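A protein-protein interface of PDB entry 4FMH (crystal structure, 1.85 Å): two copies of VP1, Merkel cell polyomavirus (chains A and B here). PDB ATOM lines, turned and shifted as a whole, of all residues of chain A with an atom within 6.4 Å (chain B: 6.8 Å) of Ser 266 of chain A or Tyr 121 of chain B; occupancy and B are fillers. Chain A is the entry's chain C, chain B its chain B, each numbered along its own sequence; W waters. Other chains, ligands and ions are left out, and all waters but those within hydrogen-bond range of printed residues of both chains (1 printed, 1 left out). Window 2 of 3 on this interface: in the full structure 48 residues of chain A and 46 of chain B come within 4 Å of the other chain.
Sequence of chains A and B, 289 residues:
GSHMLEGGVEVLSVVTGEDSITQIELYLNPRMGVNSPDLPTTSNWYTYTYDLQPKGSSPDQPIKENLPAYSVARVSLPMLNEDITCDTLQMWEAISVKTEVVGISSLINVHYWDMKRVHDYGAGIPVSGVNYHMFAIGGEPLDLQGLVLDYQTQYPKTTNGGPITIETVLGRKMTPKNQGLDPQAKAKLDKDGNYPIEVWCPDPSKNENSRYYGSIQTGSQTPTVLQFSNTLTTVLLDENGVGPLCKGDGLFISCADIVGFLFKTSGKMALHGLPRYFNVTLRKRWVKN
N of Gly 122 of chain B lies close to O of Gly 267 of chain A, 3.4 Å away.
The backbone NH (N) of Ala 123 of chain B lies within hydrogen-bond range of the side-chain sulfur (SD) of Met 269 of chain A, 3.4 Å away.
NE2 of His 119 of chain B is in hydrogen-bond range of O of Gly 267 of chain A (2.7 Å).
O of Leu 52 of chain A lies close to N of Ala 123 of chain B, 3.4 Å away.
NH1 of Arg 117 of chain B lies within hydrogen-bond range of OE1 of Gln 53 of chain A, at 2.9 Å.
NH1 of Arg 117 of chain B lies within hydrogen-bond range of O of Gly 122 of chain B, 3.0 Å away.
The side-chain hydroxyl (OG) of Ser 266 of chain A lies within hydrogen-bond range of the backbone NH (N) of Lys 268 of chain A (3.2 Å).
The backbone NH (N) of Leu 52 of chain A lies within hydrogen-bond range of the backbone carbonyl oxygen (O) of Met 269 of chain A, at 2.9 Å.
Among the printed residues, pairs that only touch across the chains: Ser 266 of chain A with Tyr 121 of chain B, Lys 268 of chain A with Tyr 121 of chain B, Gly 267 of chain A with Asp 120 of chain B, Gly 267 of chain A with Tyr 121 of chain B, Leu 52 of chain A with Gly 122 of chain B, Gln 53 of chain A with Tyr 121 of chain B, Met 269 of chain A with His 119 of chain B and Met 269 of chain A with Gly 122 of chain B.
Ser 266 of chain A touches just one residue of chain B: Tyr 121 (3.5 Å).
Tyr 121 of chain B touches four residues of chain A.
Printed residues of chain B within 4 Å of Lys 268 of chain A: Tyr 121 (3.5 Å).
Of the printed residues of chain A, His 119 of chain B touches Gly 267 and Met 269.
Printed residues of chain A within 4 Å of Gly 122 of chain B: Leu 52 (3.7 Å), Gly 267 (3.2 Å) and Met 269 (3.9 Å).
Of the printed residues of chain A, Arg 117 of chain B touches Gln 53 (2.9 Å).
Asp 114 of chain A touches none of the printed residues of chain B.
Lys 264 of chain A touches none of the printed residues of chain B.
The nearest residue of chain A that does not touch Tyr 121 of chain B is Met 269 of chain A (4.6 Å).
Of the 6 printed residues of chain B, 6 touch a printed residue of chain A.
Printed residues of chain B that touch a printed residue of chain A: Arg 117, His 119, Asp 120, Tyr 121, Gly 122 and Ala 123.
Along chain B the printed residues that touch a printed residue of chain A span positions 117 to 123.
Among the printed residues, no Asp or Glu carboxylate lies within 4 Å of a Lys or Arg side-chain nitrogen of the other chain.
No position is printed for both chains.
Of the 13 pairs that touch across the chains among the printed residues, none has its exchanged pair printed and touching as well.
Water W1 lies within hydrogen-bond range of O of Leu 52 of chain A (2.6 Å), O of Tyr 121 of chain B (2.9 Å) and N of Met 269 of chain A (2.9 Å).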
ATOM      1  N   ASP A  51     -20.887  23.320 -31.603  1.00  0.00           N
ATOM      2  CA  ASP A  51     -21.729  23.437 -30.411  1.00  0.00           C
ATOM      3  C   ASP A  51     -22.935  22.510 -30.488  1.00  0.00           C
ATOM      4  O   ASP A  51     -23.661  22.500 -31.484  1.00  0.00           O
ATOM      5  CB  ASP A  51     -22.145  24.894 -30.181  1.00  0.00           C
ATOM      6  CG  ASP A  51     -20.946  25.801 -29.955  1.00  0.00           C
ATOM      7  OD1 ASP A  51     -20.876  26.876 -30.582  1.00  0.00           O
ATOM      8  OD2 ASP A  51     -20.050  25.413 -29.174  1.00  0.00           O
ATOM      9  N   LEU A  52     -23.125  21.724 -29.431  1.00  0.00           N
ATOM     10  CA  LEU A  52     -24.221  20.761 -29.361  1.00  0.00           C
ATOM     11  C   LEU A  52     -25.415  21.378 -28.674  1.00  0.00           C
ATOM     12  O   LEU A  52     -25.303  21.829 -27.534  1.00  0.00           O
ATOM     13  CB  LEU A  52     -23.779  19.504 -28.610  1.00  0.00           C
ATOM     14  CG  LEU A  52     -22.668  18.725 -29.303  1.00  0.00           C
ATOM     15  CD1 LEU A  52     -21.857  17.947 -28.287  1.00  0.00           C
ATOM     16  CD2 LEU A  52     -23.251  17.799 -30.366  1.00  0.00           C
ATOM     17  N   GLN A  53     -26.549  21.405 -29.382  1.00  0.00           N
ATOM     18  CA  GLN A  53     -27.778  22.011 -28.874  1.00  0.00           C
ATOM     19  C   GLN A  53     -29.024  21.236 -29.296  1.00  0.00           C
ATOM     20  O   GLN A  53     -29.104  20.766 -30.426  1.00  0.00           O
ATOM     21  CB  GLN A  53     -27.925  23.453 -29.373  1.00  0.00           C
ATOM     22  CG  GLN A  53     -26.806  24.400 -28.987  1.00  0.00           C
ATOM     23  CD  GLN A  53     -27.118  25.831 -29.376  1.00  0.00           C
ATOM     24  OE1 GLN A  53     -27.864  26.521 -28.686  1.00  0.00           O
ATOM     25  NE2 GLN A  53     -26.545  26.283 -30.487  1.00  0.00           N
ATOM     26  N   ASP A 114     -11.971  31.129 -23.311  1.00  0.00           N
ATOM     27  CA  ASP A 114     -13.430  31.148 -23.454  1.00  0.00           C
ATOM     28  C   ASP A 114     -14.106  30.069 -22.607  1.00  0.00           C
ATOM     29  O   ASP A 114     -15.243  29.669 -22.870  1.00  0.00           O
ATOM     30  CB  ASP A 114     -13.842  31.024 -24.927  1.00  0.00           C
ATOM     31  CG  ASP A 114     -15.231  31.591 -25.198  1.00  0.00           C
ATOM     32  OD1 ASP A 114     -15.680  32.475 -24.444  1.00  0.00           O
ATOM     33  OD2 ASP A 114     -15.874  31.159 -26.169  1.00  0.00           O
ATOM     34  N   LYS A 116     -16.117  28.662 -19.534  1.00  0.00           N
ATOM     35  CA  LYS A 116     -17.102  29.125 -18.555  1.00  0.00           C
ATOM     36  C   LYS A 116     -16.517  28.975 -17.156  1.00  0.00           C
ATOM     37  O   LYS A 116     -15.984  27.921 -16.828  1.00  0.00           O
ATOM     38  CB  LYS A 116     -18.390  28.294 -18.674  1.00  0.00           C
ATOM     39  CG  LYS A 116     -19.480  28.661 -17.672  1.00  0.00           C
ATOM     40  CD  LYS A 116     -20.803  27.979 -18.013  1.00  0.00           C
ATOM     41  CE  LYS A 116     -21.888  28.309 -16.995  1.00  0.00           C
ATOM     42  NZ  LYS A 116     -22.200  29.771 -16.951  1.00  0.00           N
ATOM     43  N   LYS A 264     -18.140  26.497 -22.743  1.00  0.00           N
ATOM     44  CA  LYS A 264     -17.813  27.842 -23.222  1.00  0.00           C
ATOM     45  C   LYS A 264     -18.559  28.932 -22.444  1.00  0.00           C
ATOM     46  O   LYS A 264     -19.639  28.685 -21.885  1.00  0.00           O
ATOM     47  CB  LYS A 264     -18.085  27.960 -24.727  1.00  0.00           C
ATOM     48  CG  LYS A 264     -17.227  27.024 -25.569  1.00  0.00           C
ATOM     49  CD  LYS A 264     -17.655  27.000 -27.026  1.00  0.00           C
ATOM     50  CE  LYS A 264     -16.869  25.941 -27.794  1.00  0.00           C
ATOM     51  NZ  LYS A 264     -17.312  25.870 -29.206  1.00  0.00           N
ATOM     52  N   THR A 265     -17.967  30.125 -22.401  1.00  0.00           N
ATOM     53  CA  THR A 265     -18.532  31.279 -21.677  1.00  0.00           C
ATOM     54  C   THR A 265     -20.031  31.509 -21.936  1.00  0.00           C
ATOM     55  O   THR A 265     -20.812  31.700 -20.999  1.00  0.00           O
ATOM     56  CB  THR A 265     -17.764  32.566 -22.028  1.00  0.00           C
ATOM     57  OG1 THR A 265     -16.358  32.337 -21.868  1.00  0.00           O
ATOM     58  CG2 THR A 265     -18.199  33.732 -21.127  1.00  0.00           C
ATOM     59  N   SER A 266     -20.417  31.479 -23.207  1.00  0.00           N
ATOM     60  CA  SER A 266     -21.792  31.747 -23.634  1.00  0.00           C
ATOM     61  C   SER A 266     -22.811  30.756 -23.084  1.00  0.00           C
ATOM     62  O   SER A 266     -24.014  31.024 -23.105  1.00  0.00           O
ATOM     63  CB  SER A 266     -21.865  31.698 -25.156  1.00  0.00           C
ATOM     64  OG  SER A 266     -21.556  30.385 -25.605  1.00  0.00           O
ATOM     65  N   GLY A 267     -22.330  29.605 -22.617  1.00  0.00           N
ATOM     66  CA  GLY A 267     -23.198  28.505 -22.206  1.00  0.00           C
ATOM     67  C   GLY A 267     -23.102  27.349 -23.185  1.00  0.00           C
ATOM     68  O   GLY A 267     -23.519  26.232 -22.884  1.00  0.00           O
ATOM     69  N   LYS A 268     -22.532  27.614 -24.359  1.00  0.00           N
ATOM     70  CA  LYS A 268     -22.376  26.578 -25.376  1.00  0.00           C
ATOM     71  C   LYS A 268     -21.390  25.482 -24.937  1.00  0.00           C
ATOM     72  O   LYS A 268     -20.519  25.708 -24.092  1.00  0.00           O
ATOM     73  CB  LYS A 268     -22.022  27.199 -26.734  1.00  0.00           C
ATOM     74  CG  LYS A 268     -23.215  28.006 -27.270  1.00  0.00           C
ATOM     75  CD  LYS A 268     -23.028  28.547 -28.648  1.00  0.00           C
ATOM     76  CE  LYS A 268     -24.309  29.252 -29.100  1.00  0.00           C
ATOM     77  NZ  LYS A 268     -24.059  29.976 -30.363  1.00  0.00           N
ATOM     78  N   MET A 269     -21.571  24.291 -25.504  1.00  0.00           N
ATOM     79  CA  MET A 269     -20.805  23.113 -25.117  1.00  0.00           C
ATOM     80  C   MET A 269     -20.458  22.283 -26.339  1.00  0.00           C
ATOM     81  O   MET A 269     -21.301  22.059 -27.227  1.00  0.00           O
ATOM     82  CB  MET A 269     -21.613  22.248 -24.140  1.00  0.00           C
ATOM     83  CG  MET A 269     -21.901  22.919 -22.811  1.00  0.00           C
ATOM     84  SD  MET A 269     -23.242  22.156 -21.907  1.00  0.00           S
ATOM     85  CE  MET A 269     -22.649  20.464 -21.739  1.00  0.00           C
ATOM     86  N   ARG B 117     -32.076  21.408 -21.659  1.00  0.00           N
ATOM     87  CA  ARG B 117     -30.667  21.805 -21.646  1.00  0.00           C
ATOM     88  C   ARG B 117     -30.099  21.765 -20.225  1.00  0.00           C
ATOM     89  O   ARG B 117     -30.831  21.940 -19.245  1.00  0.00           O
ATOM     90  CB  ARG B 117     -30.505  23.214 -22.219  1.00  0.00           C
ATOM     91  CG  ARG B 117     -30.871  23.359 -23.691  1.00  0.00           C
ATOM     92  CD  ARG B 117     -30.743  24.814 -24.097  1.00  0.00           C
ATOM     93  NE  ARG B 117     -31.244  25.120 -25.441  1.00  0.00           N
ATOM     94  CZ  ARG B 117     -30.474  25.352 -26.502  1.00  0.00           C
ATOM     95  NH1 ARG B 117     -29.151  25.282 -26.401  1.00  0.00           N
ATOM     96  NH2 ARG B 117     -31.028  25.656 -27.676  1.00  0.00           N
ATOM     97  N   HIS B 119     -28.010  24.006 -19.169  1.00  0.00           N
ATOM     98  CA  HIS B 119     -28.113  25.441 -18.842  1.00  0.00           C
ATOM     99  C   HIS B 119     -28.415  26.191 -20.142  1.00  0.00           C
ATOM    100  O   HIS B 119     -28.434  25.579 -21.218  1.00  0.00           O
ATOM    101  CB  HIS B 119     -26.848  25.999 -18.158  1.00  0.00           C
ATOM    102  CG  HIS B 119     -25.570  25.735 -18.899  1.00  0.00           C
ATOM    103  ND1 HIS B 119     -24.498  25.092 -18.318  1.00  0.00           N
ATOM    104  CD2 HIS B 119     -25.185  26.041 -20.161  1.00  0.00           C
ATOM    105  CE1 HIS B 119     -23.509  25.007 -19.191  1.00  0.00           C
ATOM    106  NE2 HIS B 119     -23.901  25.574 -20.318  1.00  0.00           N
ATOM    107  N   ASP B 120     -28.660  27.500 -20.053  1.00  0.00           N
ATOM    108  CA  ASP B 120     -28.959  28.301 -21.248  1.00  0.00           C
ATOM    109  C   ASP B 120     -27.873  28.131 -22.313  1.00  0.00           C
ATOM    110  O   ASP B 120     -26.679  28.218 -22.009  1.00  0.00           O
ATOM    111  CB  ASP B 120     -29.119  29.783 -20.889  1.00  0.00           C
ATOM    112  CG  ASP B 120     -30.443  30.086 -20.196  1.00  0.00           C
ATOM    113  OD1 ASP B 120     -31.325  29.201 -20.132  1.00  0.00           O
ATOM    114  OD2 ASP B 120     -30.602  31.230 -19.718  1.00  0.00           O
ATOM    115  N   TYR B 121     -28.303  27.878 -23.551  1.00  0.00           N
ATOM    116  CA  TYR B 121     -27.419  27.659 -24.708  1.00  0.00           C
ATOM    117  C   TYR B 121     -26.601  26.362 -24.694  1.00  0.00           C
ATOM    118  O   TYR B 121     -25.823  26.117 -25.616  1.00  0.00           O
ATOM    119  CB  TYR B 121     -26.487  28.855 -24.938  1.00  0.00           C
ATOM    120  CG  TYR B 121     -27.240  30.149 -25.111  1.00  0.00           C
ATOM    121  CD1 TYR B 121     -27.328  31.064 -24.065  1.00  0.00           C
ATOM    122  CD2 TYR B 121     -27.881  30.448 -26.315  1.00  0.00           C
ATOM    123  CE1 TYR B 121     -28.033  32.256 -24.211  1.00  0.00           C
ATOM    124  CE2 TYR B 121     -28.587  31.643 -26.473  1.00  0.00           C
ATOM    125  CZ  TYR B 121     -28.655  32.537 -25.413  1.00  0.00           C
ATOM    126  OH  TYR B 121     -29.345  33.714 -25.552  1.00  0.00           O
ATOM    127  N   GLY B 122     -26.778  25.542 -23.663  1.00  0.00           N
ATOM    128  CA  GLY B 122     -25.987  24.322 -23.528  1.00  0.00           C
ATOM    129  C   GLY B 122     -26.545  23.133 -24.286  1.00  0.00           C
ATOM    130  O   GLY B 122     -27.563  23.237 -24.981  1.00  0.00           O
ATOM    131  N   ALA B 123     -25.853  22.004 -24.153  1.00  0.00           N
ATOM    132  CA  ALA B 123     -26.304  20.726 -24.692  1.00  0.00           C
ATOM    133  C   ALA B 123     -27.447  20.163 -23.856  1.00  0.00           C
ATOM    134  O   ALA B 123     -27.720  20.654 -22.756  1.00  0.00           O
ATOM    135  CB  ALA B 123     -25.128  19.738 -24.716  1.00  0.00           C
HETATM  136  O   HOH W   1     -24.182  24.063 -26.766  1.00  0.00           O
